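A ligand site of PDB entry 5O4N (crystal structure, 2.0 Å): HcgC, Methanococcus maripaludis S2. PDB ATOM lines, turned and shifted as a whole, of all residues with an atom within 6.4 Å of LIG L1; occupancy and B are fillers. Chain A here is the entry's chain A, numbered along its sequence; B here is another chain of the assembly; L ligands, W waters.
N of Leu 199 of chain B lies within hydrogen-bond range of O of Ser 233 of chain B, 2.8 Å away. The backbone NH of Gly 4 of chain B lies within hydrogen-bond range of the backbone carbonyl oxygen of Val 9 of chain B (2.9 Å). OG1 of Thr 174 lies within hydrogen-bond range of N of Gly 176, at 3.0 Å. The side-chain hydroxyl (OG1) of Thr 179 is in hydrogen-bond range of the side-chain hydroxyl (OG1) of Thr 174 (2.8 Å). The backbone NH (N) of Ser 175 sits at hydrogen-bond distance from the backbone carbonyl oxygen (O) of Pro 136 (3.0 Å).
Water W3 lies within hydrogen-bond range of an oxygen (O2) of LIG L1 (2.6 Å), the backbone NH (N) of Ile 5 of chain B (3.0 Å) and the side-chain carboxylate (OE2) of Glu 209 (3.1 Å). Water W4 lies within hydrogen-bond range of O3 of LIG L1, N of Met 178 and O2 of LG2 L2. Water W2 lies within hydrogen-bond range of the side-chain carboxylate (OE1) of Glu 209, a nitrogen (N1) of LIG L1 and the side-chain hydroxyl (OG) of Ser 233 of chain B. Water W5 lies within hydrogen-bond range of O of Ile 115 (2.7 Å), OG1 of Thr 6 of chain B (2.7 Å) and O2 of LIG L1 (2.7 Å). Water W1 lies within hydrogen-bond range of the side-chain carboxylate of Glu 209 (2.7 Å), an oxygen (O3) of LIG L1 (2.8 Å) and the side-chain hydroxyl of Tyr 51 (2.8 Å).
O of Thr 113 touches O1 of LIG L1 (3.6 Å). Gly 114 touches LIG L1. CB of Pro 136 touches O1 of LIG L1, at 3.5 Å. OG1 of Thr 174 touches C6 of LIG L1, at 3.6 Å. Gly 176 touches LIG L1. Met 178 touches LIG L1 (CB to O4, 3.4 Å). CD1 of Ile 5 of chain B touches O2 of LIG L1, 3.6 Å away. Val 9 of chain B touches LIG L1 (CG2 to O2, 3.5 Å). Leu 199 of chain B touches LIG L1. Hydrophobic or aromatic side chains within 4 Å of LIG L1: Ile 115, Pro 136, Met 178, Ile 5 of chain B, Val 9 of chain B and Leu 199 of chain B. 11 residues have an atom within 4 Å of LIG L1: Thr 113, Gly 114, Ile 115, Pro 136, Thr 174, Gly 176, Met 178, Thr 179, Ile 5 of chain B, Val 9 of chain B and Leu 199 of chain B. Along chain A the residues within 4 Å of LIG L1 span positions 113 to 179.
The backbone NH (N) of Thr 179 sits at hydrogen-bond distance from an oxygen (O4) of LIG L1. OG1 of Thr 179 lies within hydrogen-bond range of O4 of LIG L1. The backbone NH of Tyr 51 lies within hydrogen-bond range of an oxygen (O4) of LG2 L2 (3.3 Å). The backbone NH of Thr 177 is in hydrogen-bond range of an oxygen (O1) of LG2 L2 (3.0 Å). N of Ile 115 sits at hydrogen-bond distance from O1 of LIG L1 (2.9 Å). OG1 of Thr 177 is in hydrogen-bond range of O2 of LG2 L2, 3.0 Å away. O of Leu 112 sits at hydrogen-bond distance from N1 of LG2 L2 (2.8 Å).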
ATOM      1  N   TYR A  51      26.567   1.961   9.187  1.00  0.00           N
ATOM      2  CA  TYR A  51      25.287   1.779   9.859  1.00  0.00           C
ATOM      3  C   TYR A  51      25.223   0.374  10.484  1.00  0.00           C
ATOM      4  O   TYR A  51      25.617  -0.571   9.823  1.00  0.00           O
ATOM      5  CB  TYR A  51      24.134   2.016   8.869  1.00  0.00           C
ATOM      6  CG  TYR A  51      22.772   1.584   9.324  1.00  0.00           C
ATOM      7  CD1 TYR A  51      22.387   0.240   9.252  1.00  0.00           C
ATOM      8  CD2 TYR A  51      21.837   2.500   9.770  1.00  0.00           C
ATOM      9  CE1 TYR A  51      21.126  -0.168   9.657  1.00  0.00           C
ATOM     10  CE2 TYR A  51      20.567   2.096  10.174  1.00  0.00           C
ATOM     11  CZ  TYR A  51      20.208   0.762  10.093  1.00  0.00           C
ATOM     12  OH  TYR A  51      18.966   0.317  10.468  1.00  0.00           O
ATOM     13  N   LEU A 112      31.644  -5.187   9.635  1.00  0.00           N
ATOM     14  CA  LEU A 112      30.321  -5.137  10.277  1.00  0.00           C
ATOM     15  C   LEU A 112      29.182  -5.131   9.260  1.00  0.00           C
ATOM     16  O   LEU A 112      28.048  -4.825   9.633  1.00  0.00           O
ATOM     17  CB  LEU A 112      30.227  -3.841  11.102  1.00  0.00           C
ATOM     18  CG  LEU A 112      31.355  -3.549  12.055  1.00  0.00           C
ATOM     19  CD1 LEU A 112      31.241  -2.160  12.603  1.00  0.00           C
ATOM     20  CD2 LEU A 112      31.408  -4.579  13.167  1.00  0.00           C
ATOM     21  N   THR A 113      29.451  -5.476   8.004  1.00  0.00           N
ATOM     22  CA  THR A 113      28.424  -5.439   6.957  1.00  0.00           C
ATOM     23  C   THR A 113      27.358  -6.542   7.046  1.00  0.00           C
ATOM     24  O   THR A 113      26.225  -6.302   6.625  1.00  0.00           O
ATOM     25  CB  THR A 113      29.060  -5.395   5.582  1.00  0.00           C
ATOM     26  OG1 THR A 113      29.783  -6.605   5.363  1.00  0.00           O
ATOM     27  CG2 THR A 113      29.963  -4.173   5.416  1.00  0.00           C
ATOM     28  N   GLY A 114      27.727  -7.712   7.553  1.00  0.00           N
ATOM     29  CA  GLY A 114      26.788  -8.816   7.682  1.00  0.00           C
ATOM     30  C   GLY A 114      26.194  -9.337   6.382  1.00  0.00           C
ATOM     31  O   GLY A 114      26.907  -9.470   5.386  1.00  0.00           O
ATOM     32  N   ILE A 115      24.877  -9.625   6.405  1.00  0.00           N
ATOM     33  CA  ILE A 115      24.113 -10.190   5.268  1.00  0.00           C
ATOM     34  C   ILE A 115      24.272  -9.385   3.964  1.00  0.00           C
ATOM     35  O   ILE A 115      23.959  -8.195   3.914  1.00  0.00           O
ATOM     36  CB  ILE A 115      22.613 -10.425   5.630  1.00  0.00           C
ATOM     37  CG1 ILE A 115      22.456 -11.457   6.782  1.00  0.00           C
ATOM     38  CG2 ILE A 115      21.835 -10.907   4.405  1.00  0.00           C
ATOM     39  CD1 ILE A 115      21.185 -11.256   7.618  1.00  0.00           C
ATOM     40  N   GLY A 116      24.746 -10.066   2.920  1.00  0.00           N
ATOM     41  CA  GLY A 116      24.966  -9.476   1.614  1.00  0.00           C
ATOM     42  C   GLY A 116      26.031  -8.393   1.572  1.00  0.00           C
ATOM     43  O   GLY A 116      26.075  -7.597   0.640  1.00  0.00           O
ATOM     44  N   PRO A 136      26.192 -11.914  11.561  1.00  0.00           N
ATOM     45  CA  PRO A 136      24.833 -11.343  11.599  1.00  0.00           C
ATOM     46  C   PRO A 136      23.792 -12.317  12.152  1.00  0.00           C
ATOM     47  O   PRO A 136      22.685 -11.907  12.476  1.00  0.00           O
ATOM     48  CB  PRO A 136      24.564 -11.038  10.119  1.00  0.00           C
ATOM     49  CG  PRO A 136      25.307 -12.093   9.394  1.00  0.00           C
ATOM     50  CD  PRO A 136      26.567 -12.314  10.184  1.00  0.00           C
ATOM     51  N   LYS A 137      24.125 -13.607  12.258  1.00  0.00           N
ATOM     52  CA  LYS A 137      23.198 -14.601  12.763  1.00  0.00           C
ATOM     53  C   LYS A 137      22.870 -14.415  14.231  1.00  0.00           C
ATOM     54  O   LYS A 137      23.764 -14.110  15.020  1.00  0.00           O
ATOM     55  CB  LYS A 137      23.733 -16.024  12.559  1.00  0.00           C
ATOM     56  CG  LYS A 137      23.968 -16.406  11.087  1.00  0.00           C
ATOM     57  CD  LYS A 137      24.221 -17.902  10.895  1.00  0.00           C
ATOM     58  CE  LYS A 137      25.370 -18.488  11.693  1.00  0.00           C
ATOM     59  NZ  LYS A 137      26.692 -17.840  11.406  1.00  0.00           N
ATOM     60  N   THR A 174      18.570 -12.069  14.320  1.00  0.00           N
ATOM     61  CA  THR A 174      19.879 -11.565  13.953  1.00  0.00           C
ATOM     62  C   THR A 174      20.494 -10.855  15.145  1.00  0.00           C
ATOM     63  O   THR A 174      19.835 -10.595  16.151  1.00  0.00           O
ATOM     64  CB  THR A 174      19.847 -10.611  12.704  1.00  0.00           C
ATOM     65  OG1 THR A 174      19.631  -9.252  13.116  1.00  0.00           O
ATOM     66  CG2 THR A 174      18.856 -11.039  11.602  1.00  0.00           C
ATOM     67  N   SER A 175      21.755 -10.514  14.990  1.00  0.00           N
ATOM     68  CA  SER A 175      22.547  -9.775  15.964  1.00  0.00           C
ATOM     69  C   SER A 175      22.549  -8.300  15.593  1.00  0.00           C
ATOM     70  O   SER A 175      23.180  -7.495  16.276  1.00  0.00           O
ATOM     71  CB  SER A 175      23.977 -10.280  15.941  1.00  0.00           C
ATOM     72  OG  SER A 175      24.482 -10.155  14.611  1.00  0.00           O
ATOM     73  N   GLY A 176      21.868  -7.932  14.519  1.00  0.00           N
ATOM     74  CA  GLY A 176      21.789  -6.556  14.061  1.00  0.00           C
ATOM     75  C   GLY A 176      21.219  -5.637  15.111  1.00  0.00           C
ATOM     76  O   GLY A 176      20.275  -5.998  15.804  1.00  0.00           O
ATOM     77  N   THR A 177      21.802  -4.461  15.241  1.00  0.00           N
ATOM     78  CA  THR A 177      21.409  -3.421  16.178  1.00  0.00           C
ATOM     79  C   THR A 177      19.901  -3.127  16.035  1.00  0.00           C
ATOM     80  O   THR A 177      19.187  -3.127  17.035  1.00  0.00           O
ATOM     81  CB  THR A 177      22.206  -2.156  15.919  1.00  0.00           C
ATOM     82  OG1 THR A 177      23.577  -2.471  16.019  1.00  0.00           O
ATOM     83  CG2 THR A 177      21.905  -1.042  16.920  1.00  0.00           C
ATOM     84  N   MET A 178      19.445  -2.893  14.817  1.00  0.00           N
ATOM     85  CA  MET A 178      18.034  -2.622  14.532  1.00  0.00           C
ATOM     86  C   MET A 178      17.142  -3.778  14.973  1.00  0.00           C
ATOM     87  O   MET A 178      16.099  -3.528  15.607  1.00  0.00           O
ATOM     88  CB  MET A 178      17.837  -2.330  13.031  1.00  0.00           C
ATOM     89  CG  MET A 178      16.395  -1.970  12.622  1.00  0.00           C
ATOM     90  SD  MET A 178      15.680  -0.563  13.523  1.00  0.00           S
ATOM     91  CE  MET A 178      16.842   0.749  13.119  1.00  0.00           C
ATOM     92  N   THR A 179      17.540  -5.022  14.665  1.00  0.00           N
ATOM     93  CA  THR A 179      16.771  -6.231  15.028  1.00  0.00           C
ATOM     94  C   THR A 179      16.629  -6.321  16.532  1.00  0.00           C
ATOM     95  O   THR A 179      15.530  -6.509  17.050  1.00  0.00           O
ATOM     96  CB  THR A 179      17.415  -7.544  14.513  1.00  0.00           C
ATOM     97  OG1 THR A 179      17.430  -7.561  13.097  1.00  0.00           O
ATOM     98  CG2 THR A 179      16.665  -8.795  14.978  1.00  0.00           C
ATOM     99  N   LEU A 180      17.734  -6.175  17.218  1.00  0.00           N
ATOM    100  CA  LEU A 180      17.740  -6.228  18.683  1.00  0.00           C
ATOM    101  C   LEU A 180      16.889  -5.157  19.335  1.00  0.00           C
ATOM    102  O   LEU A 180      16.179  -5.467  20.280  1.00  0.00           O
ATOM    103  CB  LEU A 180      19.140  -6.181  19.195  1.00  0.00           C
ATOM    104  CG  LEU A 180      20.083  -7.315  18.741  1.00  0.00           C
ATOM    105  CD1 LEU A 180      21.514  -6.944  19.024  1.00  0.00           C
ATOM    106  CD2 LEU A 180      19.766  -8.593  19.411  1.00  0.00           C
ATOM    107  N   GLU A 209      15.123   1.854   8.919  1.00  0.00           N
ATOM    108  CA  GLU A 209      16.127   1.485   7.919  1.00  0.00           C
ATOM    109  C   GLU A 209      15.785   2.179   6.582  1.00  0.00           C
ATOM    110  O   GLU A 209      16.689   2.626   5.881  1.00  0.00           O
ATOM    111  CB  GLU A 209      16.161  -0.057   7.799  1.00  0.00           C
ATOM    112  CG  GLU A 209      17.044  -0.651   6.708  1.00  0.00           C
ATOM    113  CD  GLU A 209      16.819  -2.139   6.574  1.00  0.00           C
ATOM    114  OE1 GLU A 209      17.024  -2.848   7.579  1.00  0.00           O
ATOM    115  OE2 GLU A 209      16.346  -2.597   5.498  1.00  0.00           O
ATOM    116  N   GLY B   4      16.193  -4.022   0.964  1.00  0.00           N
ATOM    117  CA  GLY B   4      16.547  -3.263   2.151  1.00  0.00           C
ATOM    118  C   GLY B   4      17.884  -2.560   1.976  1.00  0.00           C
ATOM    119  O   GLY B   4      18.028  -1.728   1.085  1.00  0.00           O
ATOM    120  N   ILE B   5      18.869  -2.910   2.817  1.00  0.00           N
ATOM    121  CA  ILE B   5      20.215  -2.322   2.793  1.00  0.00           C
ATOM    122  C   ILE B   5      20.976  -2.740   1.527  1.00  0.00           C
ATOM    123  O   ILE B   5      21.736  -1.946   0.956  1.00  0.00           O
ATOM    124  CB  ILE B   5      20.949  -2.653   4.125  1.00  0.00           C
ATOM    125  CG1 ILE B   5      20.199  -1.964   5.281  1.00  0.00           C
ATOM    126  CG2 ILE B   5      22.387  -2.208   4.092  1.00  0.00           C
ATOM    127  CD1 ILE B   5      20.454  -2.492   6.704  1.00  0.00           C
ATOM    128  N   THR B   6      20.776  -3.979   1.093  1.00  0.00           N
ATOM    129  CA  THR B   6      21.394  -4.549  -0.105  1.00  0.00           C
ATOM    130  C   THR B   6      20.326  -5.382  -0.774  1.00  0.00           C
ATOM    131  O   THR B   6      19.232  -5.549  -0.217  1.00  0.00           O
ATOM    132  CB  THR B   6      22.635  -5.450   0.225  1.00  0.00           C
ATOM    133  OG1 THR B   6      22.202  -6.685   0.789  1.00  0.00           O
ATOM    134  CG2 THR B   6      23.656  -4.752   1.101  1.00  0.00           C
ATOM    135  N   VAL B   9      18.555  -8.719   0.990  1.00  0.00           N
ATOM    136  CA  VAL B   9      17.460  -8.624   1.951  1.00  0.00           C
ATOM    137  C   VAL B   9      16.272  -7.925   1.319  1.00  0.00           C
ATOM    138  O   VAL B   9      16.424  -6.905   0.680  1.00  0.00           O
ATOM    139  CB  VAL B   9      17.938  -7.913   3.245  1.00  0.00           C
ATOM    140  CG1 VAL B   9      16.827  -7.819   4.285  1.00  0.00           C
ATOM    141  CG2 VAL B   9      19.159  -8.620   3.834  1.00  0.00           C
ATOM    142  N   LEU B 199      14.084 -11.444   9.271  1.00  0.00           N
ATOM    143  CA  LEU B 199      15.122 -10.839  10.107  1.00  0.00           C
ATOM    144  C   LEU B 199      14.420 -10.115  11.263  1.00  0.00           C
ATOM    145  O   LEU B 199      14.776 -10.283  12.441  1.00  0.00           O
ATOM    146  CB  LEU B 199      15.960  -9.839   9.322  1.00  0.00           C
ATOM    147  CG  LEU B 199      16.670 -10.276   8.053  1.00  0.00           C
ATOM    148  CD1 LEU B 199      17.734  -9.245   7.676  1.00  0.00           C
ATOM    149  CD2 LEU B 199      17.328 -11.612   8.198  1.00  0.00           C
ATOM    150  N   TYR B 200      13.442  -9.259  10.929  1.00  0.00           N
ATOM    151  CA  TYR B 200      12.705  -8.512  11.929  1.00  0.00           C
ATOM    152  C   TYR B 200      11.379  -8.056  11.347  1.00  0.00           C
ATOM    153  O   TYR B 200      11.219  -7.997  10.129  1.00  0.00           O
ATOM    154  CB  TYR B 200      13.527  -7.382  12.618  1.00  0.00           C
ATOM    155  CG  TYR B 200      13.864  -6.218  11.724  1.00  0.00           C
ATOM    156  CD1 TYR B 200      12.932  -5.217  11.469  1.00  0.00           C
ATOM    157  CD2 TYR B 200      15.122  -6.101  11.152  1.00  0.00           C
ATOM    158  CE1 TYR B 200      13.240  -4.139  10.636  1.00  0.00           C
ATOM    159  CE2 TYR B 200      15.443  -5.020  10.325  1.00  0.00           C
ATOM    160  CZ  TYR B 200      14.502  -4.036  10.081  1.00  0.00           C
ATOM    161  OH  TYR B 200      14.769  -2.947   9.290  1.00  0.00           O
ATOM    162  N   SER B 233      11.360  -7.401   7.159  1.00  0.00           N
ATOM    163  CA  SER B 233      12.690  -7.477   6.565  1.00  0.00           C
ATOM    164  C   SER B 233      12.969  -8.994   6.514  1.00  0.00           C
ATOM    165  O   SER B 233      12.896  -9.665   7.538  1.00  0.00           O
ATOM    166  CB  SER B 233      13.731  -6.765   7.395  1.00  0.00           C
ATOM    167  OG  SER B 233      15.016  -6.993   6.839  1.00  0.00           O
HETATM  168  C1  LIG L   1      22.427  -7.491   8.330  1.00  0.00           C
HETATM  169  C2  LIG L   1      21.553  -7.419   9.420  1.00  0.00           C
HETATM  170  C3  LIG L   1      20.295  -6.825   9.200  1.00  0.00           C
HETATM  171  C4  LIG L   1      20.820  -6.429   6.924  1.00  0.00           C
HETATM  172  O1  LIG L   1      23.661  -8.051   8.465  1.00  0.00           O
HETATM  173  N1  LIG L   1      19.975  -6.347   7.968  1.00  0.00           N
HETATM  174  C5  LIG L   1      22.073  -6.992   7.088  1.00  0.00           C
HETATM  175  O2  LIG L   1      20.442  -5.927   5.725  1.00  0.00           O
HETATM  176  C6  LIG L   1      21.969  -7.960  10.777  1.00  0.00           C
HETATM  177  C7  LIG L   1      19.263  -6.666  10.269  1.00  0.00           C
HETATM  178  C8  LIG L   1      19.575  -5.374  11.015  1.00  0.00           C
HETATM  179  O3  LIG L   1      20.175  -4.414  10.458  1.00  0.00           O
HETATM  180  O4  LIG L   1      19.182  -5.358  12.200  1.00  0.00           O
HETATM  181  N1  LG2 L   2      26.067  -4.985  11.588  1.00  0.00           N
HETATM  182  C1  LG2 L   2      25.248  -3.739  11.507  1.00  0.00           C
HETATM  183  C2  LG2 L   2      24.194  -3.828  10.399  1.00  0.00           C
HETATM  184  C3  LG2 L   2      24.821  -4.114   9.038  1.00  0.00           C
HETATM  185  S1  LG2 L   2      24.037  -3.194   7.759  1.00  0.00           S
HETATM  186  C4  LG2 L   2      24.551  -3.474  12.809  1.00  0.00           C
HETATM  187  O1  LG2 L   2      24.339  -4.405  13.605  1.00  0.00           O
HETATM  188  O2  LG2 L   2      24.191  -2.326  13.070  1.00  0.00           O
HETATM  189  C5  LG2 L   2      25.220  -3.130   6.449  1.00  0.00           C
HETATM  190  C6  LG2 L   2      26.038  -1.825   6.478  1.00  0.00           C
HETATM  191  O3  LG2 L   2      27.232  -2.021   5.693  1.00  0.00           O
HETATM  192  C7  LG2 L   2      25.294  -0.673   5.779  1.00  0.00           C
HETATM  193  O4  LG2 L   2      25.832   0.577   6.256  1.00  0.00           O
HETATM  194  C8  LG2 L   2      25.656  -0.882   4.308  1.00  0.00           C
HETATM  195  O5  LG2 L   2      25.494   0.293   3.493  1.00  0.00           O
HETATM  196  C9  LG2 L   2      27.136  -1.323   4.437  1.00  0.00           C
HETATM  197  N2  LG2 L   2      27.605  -2.228   3.364  1.00  0.00           N
HETATM  198  C10 LG2 L   2      26.903  -3.217   2.739  1.00  0.00           C
HETATM  199  N3  LG2 L   2      27.686  -3.840   1.829  1.00  0.00           N
HETATM  200  C11 LG2 L   2      28.899  -3.272   1.884  1.00  0.00           C
HETATM  201  C12 LG2 L   2      30.206  -3.442   1.201  1.00  0.00           C
HETATM  202  N4  LG2 L   2      30.367  -4.393   0.243  1.00  0.00           N
HETATM  203  N5  LG2 L   2      31.231  -2.628   1.565  1.00  0.00           N
HETATM  204  C13 LG2 L   2      31.116  -1.675   2.514  1.00  0.00           C
HETATM  205  N6  LG2 L   2      29.954  -1.473   3.167  1.00  0.00           N
HETATM  206  C14 LG2 L   2      28.839  -2.204   2.897  1.00  0.00           C
HETATM  207  O   HOH W   1      18.397  -2.373   9.853  1.00  0.00           O
HETATM  208  O   HOH W   2      17.450  -5.437   7.537  1.00  0.00           O
HETATM  209  O   HOH W   3      18.225  -4.943   4.878  1.00  0.00           O
HETATM  210  O   HOH W   4      21.051  -2.672  12.317  1.00  0.00           O
HETATM  211  O   HOH W   5      21.860  -6.584   3.477  1.00  0.00           O
